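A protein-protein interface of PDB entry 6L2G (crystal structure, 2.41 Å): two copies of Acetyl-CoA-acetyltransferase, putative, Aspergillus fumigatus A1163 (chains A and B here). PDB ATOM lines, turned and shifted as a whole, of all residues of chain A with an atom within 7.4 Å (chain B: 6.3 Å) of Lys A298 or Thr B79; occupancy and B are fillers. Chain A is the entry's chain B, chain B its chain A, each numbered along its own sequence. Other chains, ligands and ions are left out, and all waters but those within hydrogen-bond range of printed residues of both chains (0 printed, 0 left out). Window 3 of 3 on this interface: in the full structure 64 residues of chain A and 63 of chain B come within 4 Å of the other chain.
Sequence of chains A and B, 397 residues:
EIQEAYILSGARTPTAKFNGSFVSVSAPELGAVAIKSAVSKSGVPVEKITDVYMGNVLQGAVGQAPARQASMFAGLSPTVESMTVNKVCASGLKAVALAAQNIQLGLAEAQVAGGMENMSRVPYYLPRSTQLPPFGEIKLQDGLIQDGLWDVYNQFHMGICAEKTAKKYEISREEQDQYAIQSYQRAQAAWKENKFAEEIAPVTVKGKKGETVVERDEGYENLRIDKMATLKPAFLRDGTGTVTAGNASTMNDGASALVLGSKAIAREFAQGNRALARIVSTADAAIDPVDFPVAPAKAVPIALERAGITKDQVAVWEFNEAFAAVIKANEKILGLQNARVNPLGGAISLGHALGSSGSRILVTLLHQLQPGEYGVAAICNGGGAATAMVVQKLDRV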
ATOM      1  N   ALA A 283     -27.307  -2.523  12.245  1.00  0.00           N
ATOM      2  CA  ALA A 283     -27.949  -1.628  13.216  1.00  0.00           C
ATOM      3  C   ALA A 283     -26.919  -1.210  14.251  1.00  0.00           C
ATOM      4  O   ALA A 283     -26.105  -2.068  14.658  1.00  0.00           O
ATOM      5  CB  ALA A 283     -29.129  -2.324  13.843  1.00  0.00           C
ATOM      6  N   ASP A 284     -26.973   0.072  14.620  1.00  0.00           N
ATOM      7  CA  ASP A 284     -26.232   0.667  15.755  1.00  0.00           C
ATOM      8  C   ASP A 284     -27.249   0.982  16.864  1.00  0.00           C
ATOM      9  O   ASP A 284     -28.412   1.253  16.563  1.00  0.00           O
ATOM     10  CB  ASP A 284     -25.456   1.899  15.289  1.00  0.00           C
ATOM     11  CG  ASP A 284     -24.404   1.628  14.222  1.00  0.00           C
ATOM     12  OD1 ASP A 284     -23.842   0.520  14.211  1.00  0.00           O
ATOM     13  OD2 ASP A 284     -24.152   2.530  13.406  1.00  0.00           O
ATOM     14  N   ALA A 285     -26.835   0.953  18.124  1.00  0.00           N
ATOM     15  CA  ALA A 285     -27.698   1.369  19.241  1.00  0.00           C
ATOM     16  C   ALA A 285     -26.818   1.798  20.404  1.00  0.00           C
ATOM     17  O   ALA A 285     -25.730   1.272  20.530  1.00  0.00           O
ATOM     18  CB  ALA A 285     -28.647   0.253  19.616  1.00  0.00           C
ATOM     19  N   ALA A 286     -27.305   2.738  21.209  1.00  0.00           N
ATOM     20  CA  ALA A 286     -26.613   3.280  22.394  1.00  0.00           C
ATOM     21  C   ALA A 286     -27.591   3.372  23.557  1.00  0.00           C
ATOM     22  O   ALA A 286     -28.783   3.547  23.318  1.00  0.00           O
ATOM     23  CB  ALA A 286     -26.052   4.633  22.073  1.00  0.00           C
ATOM     24  N   ILE A 287     -27.057   3.300  24.774  1.00  0.00           N
ATOM     25  CA  ILE A 287     -27.761   3.559  26.062  1.00  0.00           C
ATOM     26  C   ILE A 287     -26.761   4.302  26.934  1.00  0.00           C
ATOM     27  O   ILE A 287     -25.706   4.694  26.382  1.00  0.00           O
ATOM     28  CB  ILE A 287     -28.198   2.223  26.673  1.00  0.00           C
ATOM     29  CG1 ILE A 287     -26.975   1.380  27.068  1.00  0.00           C
ATOM     30  CG2 ILE A 287     -29.125   1.483  25.708  1.00  0.00           C
ATOM     31  CD1 ILE A 287     -27.301  -0.056  27.423  1.00  0.00           C
ATOM     32  N   ASP A 288     -27.047   4.467  28.227  1.00  0.00           N
ATOM     33  CA  ASP A 288     -26.094   5.032  29.224  1.00  0.00           C
ATOM     34  C   ASP A 288     -24.710   4.406  29.060  1.00  0.00           C
ATOM     35  O   ASP A 288     -24.603   3.188  28.909  1.00  0.00           O
ATOM     36  CB  ASP A 288     -26.581   4.817  30.657  1.00  0.00           C
ATOM     37  CG  ASP A 288     -27.678   5.787  31.038  1.00  0.00           C
ATOM     38  OD1 ASP A 288     -27.346   6.966  31.284  1.00  0.00           O
ATOM     39  OD2 ASP A 288     -28.851   5.367  31.032  1.00  0.00           O
ATOM     40  N   VAL A 294     -24.488  -4.246  27.744  1.00  0.00           N
ATOM     41  CA  VAL A 294     -25.824  -4.797  27.351  1.00  0.00           C
ATOM     42  C   VAL A 294     -26.369  -4.074  26.113  1.00  0.00           C
ATOM     43  O   VAL A 294     -27.479  -4.441  25.696  1.00  0.00           O
ATOM     44  CB  VAL A 294     -26.840  -4.757  28.512  1.00  0.00           C
ATOM     45  CG1 VAL A 294     -26.421  -5.700  29.630  1.00  0.00           C
ATOM     46  CG2 VAL A 294     -27.076  -3.346  29.046  1.00  0.00           C
ATOM     47  N   ALA A 295     -25.623  -3.127  25.526  1.00  0.00           N
ATOM     48  CA  ALA A 295     -25.991  -2.413  24.273  1.00  0.00           C
ATOM     49  C   ALA A 295     -26.286  -3.403  23.146  1.00  0.00           C
ATOM     50  O   ALA A 295     -27.221  -3.206  22.366  1.00  0.00           O
ATOM     51  CB  ALA A 295     -24.905  -1.449  23.876  1.00  0.00           C
ATOM     52  N   PRO A 296     -25.502  -4.490  22.984  1.00  0.00           N
ATOM     53  CA  PRO A 296     -25.759  -5.445  21.903  1.00  0.00           C
ATOM     54  C   PRO A 296     -27.195  -5.998  21.900  1.00  0.00           C
ATOM     55  O   PRO A 296     -27.733  -6.212  20.814  1.00  0.00           O
ATOM     56  CB  PRO A 296     -24.717  -6.537  22.164  1.00  0.00           C
ATOM     57  CG  PRO A 296     -23.584  -5.784  22.823  1.00  0.00           C
ATOM     58  CD  PRO A 296     -24.296  -4.828  23.756  1.00  0.00           C
ATOM     59  N   ALA A 297     -27.771  -6.191  23.094  1.00  0.00           N
ATOM     60  CA  ALA A 297     -29.165  -6.652  23.326  1.00  0.00           C
ATOM     61  C   ALA A 297     -30.152  -5.632  22.752  1.00  0.00           C
ATOM     62  O   ALA A 297     -31.238  -6.066  22.324  1.00  0.00           O
ATOM     63  CB  ALA A 297     -29.424  -6.881  24.798  1.00  0.00           C
ATOM     64  N   LYS A 298     -29.778  -4.349  22.698  1.00  0.00           N
ATOM     65  CA  LYS A 298     -30.558  -3.301  21.978  1.00  0.00           C
ATOM     66  C   LYS A 298     -30.332  -3.348  20.451  1.00  0.00           C
ATOM     67  O   LYS A 298     -31.297  -3.142  19.708  1.00  0.00           O
ATOM     68  CB  LYS A 298     -30.230  -1.910  22.509  1.00  0.00           C
ATOM     69  CG  LYS A 298     -31.189  -0.846  21.992  1.00  0.00           C
ATOM     70  CD  LYS A 298     -31.049   0.518  22.639  1.00  0.00           C
ATOM     71  CE  LYS A 298     -31.907   1.547  21.943  1.00  0.00           C
ATOM     72  NZ  LYS A 298     -31.422   2.921  22.198  1.00  0.00           N
ATOM     73  N   ALA A 299     -29.110  -3.571  19.977  1.00  0.00           N
ATOM     74  CA  ALA A 299     -28.762  -3.524  18.536  1.00  0.00           C
ATOM     75  C   ALA A 299     -29.275  -4.770  17.810  1.00  0.00           C
ATOM     76  O   ALA A 299     -29.685  -4.678  16.635  1.00  0.00           O
ATOM     77  CB  ALA A 299     -27.268  -3.413  18.374  1.00  0.00           C
ATOM     78  N   VAL A 300     -29.192  -5.926  18.454  1.00  0.00           N
ATOM     79  CA  VAL A 300     -29.509  -7.222  17.795  1.00  0.00           C
ATOM     80  C   VAL A 300     -30.962  -7.232  17.304  1.00  0.00           C
ATOM     81  O   VAL A 300     -31.202  -7.557  16.141  1.00  0.00           O
ATOM     82  CB  VAL A 300     -29.146  -8.407  18.707  1.00  0.00           C
ATOM     83  CG1 VAL A 300     -29.868  -9.676  18.289  1.00  0.00           C
ATOM     84  CG2 VAL A 300     -27.643  -8.616  18.715  1.00  0.00           C
ATOM     85  N   PRO A 301     -31.979  -6.876  18.118  1.00  0.00           N
ATOM     86  CA  PRO A 301     -33.371  -6.897  17.654  1.00  0.00           C
ATOM     87  C   PRO A 301     -33.621  -5.917  16.504  1.00  0.00           C
ATOM     88  O   PRO A 301     -34.350  -6.241  15.583  1.00  0.00           O
ATOM     89  CB  PRO A 301     -34.217  -6.494  18.870  1.00  0.00           C
ATOM     90  CG  PRO A 301     -33.294  -6.730  20.056  1.00  0.00           C
ATOM     91  CD  PRO A 301     -31.882  -6.514  19.535  1.00  0.00           C
ATOM     92  N   ILE A 302     -32.992  -4.747  16.545  1.00  0.00           N
ATOM     93  CA  ILE A 302     -33.122  -3.785  15.413  1.00  0.00           C
ATOM     94  C   ILE A 302     -32.606  -4.452  14.137  1.00  0.00           C
ATOM     95  O   ILE A 302     -33.303  -4.371  13.104  1.00  0.00           O
ATOM     96  CB  ILE A 302     -32.427  -2.452  15.699  1.00  0.00           C
ATOM     97  CG1 ILE A 302     -33.016  -1.793  16.949  1.00  0.00           C
ATOM     98  CG2 ILE A 302     -32.540  -1.567  14.470  1.00  0.00           C
ATOM     99  CD1 ILE A 302     -32.336  -0.499  17.367  1.00  0.00           C
ATOM    100  N   ALA A 303     -31.460  -5.130  14.216  1.00  0.00           N
ATOM    101  CA  ALA A 303     -30.833  -5.814  13.061  1.00  0.00           C
ATOM    102  C   ALA A 303     -31.734  -6.966  12.609  1.00  0.00           C
ATOM    103  O   ALA A 303     -31.956  -7.126  11.378  1.00  0.00           O
ATOM    104  CB  ALA A 303     -29.443  -6.287  13.411  1.00  0.00           C
ATOM    105  N   ASN A 330     -25.897 -10.828  27.966  1.00  0.00           N
ATOM    106  CA  ASN A 330     -26.516 -10.751  26.617  1.00  0.00           C
ATOM    107  C   ASN A 330     -27.215 -12.077  26.289  1.00  0.00           C
ATOM    108  O   ASN A 330     -28.296 -12.039  25.664  1.00  0.00           O
ATOM    109  CB  ASN A 330     -25.497 -10.329  25.557  1.00  0.00           C
ATOM    110  CG  ASN A 330     -25.225  -8.842  25.611  1.00  0.00           C
ATOM    111  OD1 ASN A 330     -26.127  -8.043  25.364  1.00  0.00           O
ATOM    112  ND2 ASN A 330     -24.006  -8.453  25.955  1.00  0.00           N
ATOM    113  N   ILE A 333     -30.694 -11.877  28.248  1.00  0.00           N
ATOM    114  CA  ILE A 333     -31.699 -10.913  27.704  1.00  0.00           C
ATOM    115  C   ILE A 333     -32.295 -11.438  26.389  1.00  0.00           C
ATOM    116  O   ILE A 333     -33.488 -11.193  26.145  1.00  0.00           O
ATOM    117  CB  ILE A 333     -31.061  -9.524  27.514  1.00  0.00           C
ATOM    118  CG1 ILE A 333     -30.643  -8.891  28.843  1.00  0.00           C
ATOM    119  CG2 ILE A 333     -31.988  -8.609  26.733  1.00  0.00           C
ATOM    120  CD1 ILE A 333     -29.624  -7.786  28.692  1.00  0.00           C
ATOM    121  N   LEU A 334     -31.498 -12.080  25.534  1.00  0.00           N
ATOM    122  CA  LEU A 334     -31.935 -12.465  24.162  1.00  0.00           C
ATOM    123  C   LEU A 334     -32.367 -13.937  24.153  1.00  0.00           C
ATOM    124  O   LEU A 334     -32.797 -14.428  23.078  1.00  0.00           O
ATOM    125  CB  LEU A 334     -30.789 -12.222  23.172  1.00  0.00           C
ATOM    126  CG  LEU A 334     -30.342 -10.767  22.988  1.00  0.00           C
ATOM    127  CD1 LEU A 334     -29.064 -10.707  22.163  1.00  0.00           C
ATOM    128  CD2 LEU A 334     -31.420  -9.932  22.318  1.00  0.00           C
ATOM    129  N   GLY A 384     -21.173   3.376  25.671  1.00  0.00           N
ATOM    130  CA  GLY A 384     -22.490   2.738  25.880  1.00  0.00           C
ATOM    131  C   GLY A 384     -23.214   2.341  24.594  1.00  0.00           C
ATOM    132  O   GLY A 384     -24.429   2.512  24.540  1.00  0.00           O
ATOM    133  N   ALA A 386     -23.225  -0.212  20.562  1.00  0.00           N
ATOM    134  CA  ALA A 386     -22.987  -1.543  19.980  1.00  0.00           C
ATOM    135  C   ALA A 386     -23.397  -1.522  18.513  1.00  0.00           C
ATOM    136  O   ALA A 386     -24.286  -0.744  18.171  1.00  0.00           O
ATOM    137  CB  ALA A 386     -23.758  -2.580  20.749  1.00  0.00           C
ATOM    138  N   ALA A 388     -24.365  -4.425  15.414  1.00  0.00           N
ATOM    139  CA  ALA A 388     -24.751  -5.798  15.039  1.00  0.00           C
ATOM    140  C   ALA A 388     -25.002  -5.829  13.538  1.00  0.00           C
ATOM    141  O   ALA A 388     -25.616  -4.888  13.028  1.00  0.00           O
ATOM    142  CB  ALA A 388     -25.980  -6.230  15.805  1.00  0.00           C
ATOM    143  N   THR B  50     -30.939  10.910  15.791  1.00  0.00           N
ATOM    144  CA  THR B  50     -30.555   9.566  16.304  1.00  0.00           C
ATOM    145  C   THR B  50     -29.046   9.315  16.219  1.00  0.00           C
ATOM    146  O   THR B  50     -28.628   8.317  16.788  1.00  0.00           O
ATOM    147  CB  THR B  50     -31.355   8.460  15.615  1.00  0.00           C
ATOM    148  OG1 THR B  50     -31.222   8.658  14.216  1.00  0.00           O
ATOM    149  CG2 THR B  50     -32.816   8.454  16.012  1.00  0.00           C
ATOM    150  N   ARG B  68     -18.728  10.973  20.794  1.00  0.00           N
ATOM    151  CA  ARG B  68     -19.687  10.610  21.875  1.00  0.00           C
ATOM    152  C   ARG B  68     -19.626  11.718  22.928  1.00  0.00           C
ATOM    153  O   ARG B  68     -20.710  12.172  23.360  1.00  0.00           O
ATOM    154  CB  ARG B  68     -19.374   9.229  22.453  1.00  0.00           C
ATOM    155  CG  ARG B  68     -20.266   8.799  23.605  1.00  0.00           C
ATOM    156  CD  ARG B  68     -21.712   8.666  23.220  1.00  0.00           C
ATOM    157  NE  ARG B  68     -22.457   7.845  24.164  1.00  0.00           N
ATOM    158  CZ  ARG B  68     -23.766   7.604  24.098  1.00  0.00           C
ATOM    159  NH1 ARG B  68     -24.500   8.145  23.135  1.00  0.00           N
ATOM    160  NH2 ARG B  68     -24.338   6.831  25.007  1.00  0.00           N
ATOM    161  N   LEU B  76     -27.390  15.944  24.414  1.00  0.00           N
ATOM    162  CA  LEU B  76     -28.145  14.929  23.629  1.00  0.00           C
ATOM    163  C   LEU B  76     -28.308  13.656  24.475  1.00  0.00           C
ATOM    164  O   LEU B  76     -27.477  13.383  25.366  1.00  0.00           O
ATOM    165  CB  LEU B  76     -27.444  14.666  22.294  1.00  0.00           C
ATOM    166  CG  LEU B  76     -27.962  15.438  21.076  1.00  0.00           C
ATOM    167  CD1 LEU B  76     -28.409  16.834  21.434  1.00  0.00           C
ATOM    168  CD2 LEU B  76     -26.913  15.488  19.972  1.00  0.00           C
ATOM    169  N   SER B  77     -29.376  12.909  24.216  1.00  0.00           N
ATOM    170  CA  SER B  77     -29.710  11.650  24.926  1.00  0.00           C
ATOM    171  C   SER B  77     -28.590  10.617  24.742  1.00  0.00           C
ATOM    172  O   SER B  77     -28.020  10.474  23.662  1.00  0.00           O
ATOM    173  CB  SER B  77     -31.046  11.124  24.451  1.00  0.00           C
ATOM    174  OG  SER B  77     -31.207   9.764  24.834  1.00  0.00           O
ATOM    175  N   PRO B  78     -28.260   9.824  25.783  1.00  0.00           N
ATOM    176  CA  PRO B  78     -27.362   8.686  25.614  1.00  0.00           C
ATOM    177  C   PRO B  78     -27.858   7.631  24.608  1.00  0.00           C
ATOM    178  O   PRO B  78     -27.064   6.770  24.286  1.00  0.00           O
ATOM    179  CB  PRO B  78     -27.242   8.042  27.008  1.00  0.00           C
ATOM    180  CG  PRO B  78     -28.208   8.797  27.927  1.00  0.00           C
ATOM    181  CD  PRO B  78     -28.719   9.998  27.166  1.00  0.00           C
ATOM    182  N   THR B  79     -29.122   7.696  24.154  1.00  0.00           N
ATOM    183  CA  THR B  79     -29.677   6.805  23.087  1.00  0.00           C
ATOM    184  C   THR B  79     -29.132   7.226  21.716  1.00  0.00           C
ATOM    185  O   THR B  79     -29.269   6.442  20.769  1.00  0.00           O
ATOM    186  CB  THR B  79     -31.218   6.783  23.059  1.00  0.00           C
ATOM    187  OG1 THR B  79     -31.745   8.112  23.068  1.00  0.00           O
ATOM    188  CG2 THR B  79     -31.806   6.031  24.229  1.00  0.00           C
ATOM    189  N   VAL B  80     -28.554   8.422  21.609  1.00  0.00           N
ATOM    190  CA  VAL B  80     -28.036   8.954  20.320  1.00  0.00           C
ATOM    191  C   VAL B  80     -26.719   8.248  20.016  1.00  0.00           C
ATOM    192  O   VAL B  80     -25.832   8.260  20.879  1.00  0.00           O
ATOM    193  CB  VAL B  80     -27.840  10.476  20.342  1.00  0.00           C
ATOM    194  CG1 VAL B  80     -27.278  10.964  19.017  1.00  0.00           C
ATOM    195  CG2 VAL B  80     -29.140  11.194  20.690  1.00  0.00           C
ATOM    196  N   GLU B  81     -26.604   7.688  18.817  1.00  0.00           N
ATOM    197  CA  GLU B  81     -25.411   6.915  18.401  1.00  0.00           C
ATOM    198  C   GLU B  81     -24.368   7.903  17.883  1.00  0.00           C
ATOM    199  O   GLU B  81     -24.711   9.062  17.631  1.00  0.00           O
ATOM    200  CB  GLU B  81     -25.784   5.803  17.419  1.00  0.00           C
ATOM    201  CG  GLU B  81     -25.647   4.412  18.043  1.00  0.00           C
ATOM    202  CD  GLU B  81     -24.232   3.894  18.351  1.00  0.00           C
ATOM    203  OE1 GLU B  81     -23.283   4.709  18.514  1.00  0.00           O
ATOM    204  OE2 GLU B  81     -24.071   2.650  18.427  1.00  0.00           O
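Hydrophobic or aromatic side chains of chain A that line the printed part of chain B: Ala A286. Of the 8 printed residues of chain B, 5 touch a printed residue of chain A. Printed residues of chain B that touch a printed residue of chain A: Arg B68, Pro B78, Thr B79, Val B80 and Glu B81. Among the printed residues, no Asp or Glu carboxylate lies within 4 Å of a Lys or Arg side-chain nitrogen of the other chain.
Of chain B, only Thr B79 comes within 4 Å of Lys A298. Of the printed residues of chain A, Thr B79 touches Ala A286 (3.4 Å) and Lys A298 (3.7 Å). Of the printed residues of chain B, Ala A386 touches Glu B81. Printed residues of chain A within 4 Å of Val B80: Ala A286. Of the printed residues of chain A, Arg B68 touches Ala A286 and Ile A287. Gly A384 touches none of the printed residues of chain B. Val A300 touches none of the printed residues of chain B. The nearest residue of chain B that does not touch Lys A298 is Pro B78 (6.2 Å). The nearest residue of chain A that does not touch Thr B79 is Ile A287 (4.7 Å).
No position is printed for both chains.
Asp A284 touches Glu B81 (CB to OE2, 3.5 Å). NH1 of Arg B68 touches CB of Ala A286, at 3.98 Å. Ala A286 touches Pro B78. Thr B79 touches Ala A286. CB of Ala A286 touches O of Val B80, at 3.8 Å. N of Ala A286 touches CG of Glu B81 (3.9 Å). Asp A288 touches Pro B78 (N to CB, 3.8 Å). Thr B79 touches Lys A298 (CG2 to NZ, 3.7 Å).
NH2 of Arg B68 is in hydrogen-bond range of O of Ile A287, 2.9 Å away. The side-chain carboxylate of Glu B81 sits close to the backbone carbonyl oxygen of Ala A386 (3.4 Å). O of Ile A287 lies close to O of Pro B78 (3.2 Å). The side-chain carboxylate (OE2) of Glu B81 sits at hydrogen-bond distance from the backbone NH (N) of Ala A285.
The side-chain hydroxyl (OG1) of Thr B79 lies within hydrogen-bond range of the side-chain hydroxyl (OG) of Ser B77 (2.5 Å). O of Val B80 lies within hydrogen-bond range of NH1 of Arg B68, 2.6 Å away. The backbone carbonyl oxygen of Gly A384 lies within hydrogen-bond range of the backbone NH of Ile A287 (2.8 Å). The backbone carbonyl oxygen of Thr B50 sits at hydrogen-bond distance from the backbone NH of Glu B81 (2.9 Å). The backbone carbonyl oxygen of Ala A285 sits at hydrogen-bond distance from the backbone NH of Ala A386 (2.9 Å). The side-chain amino group (NZ) of Lys A298 sits at hydrogen-bond distance from the backbone carbonyl oxygen (O) of Ala A286.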
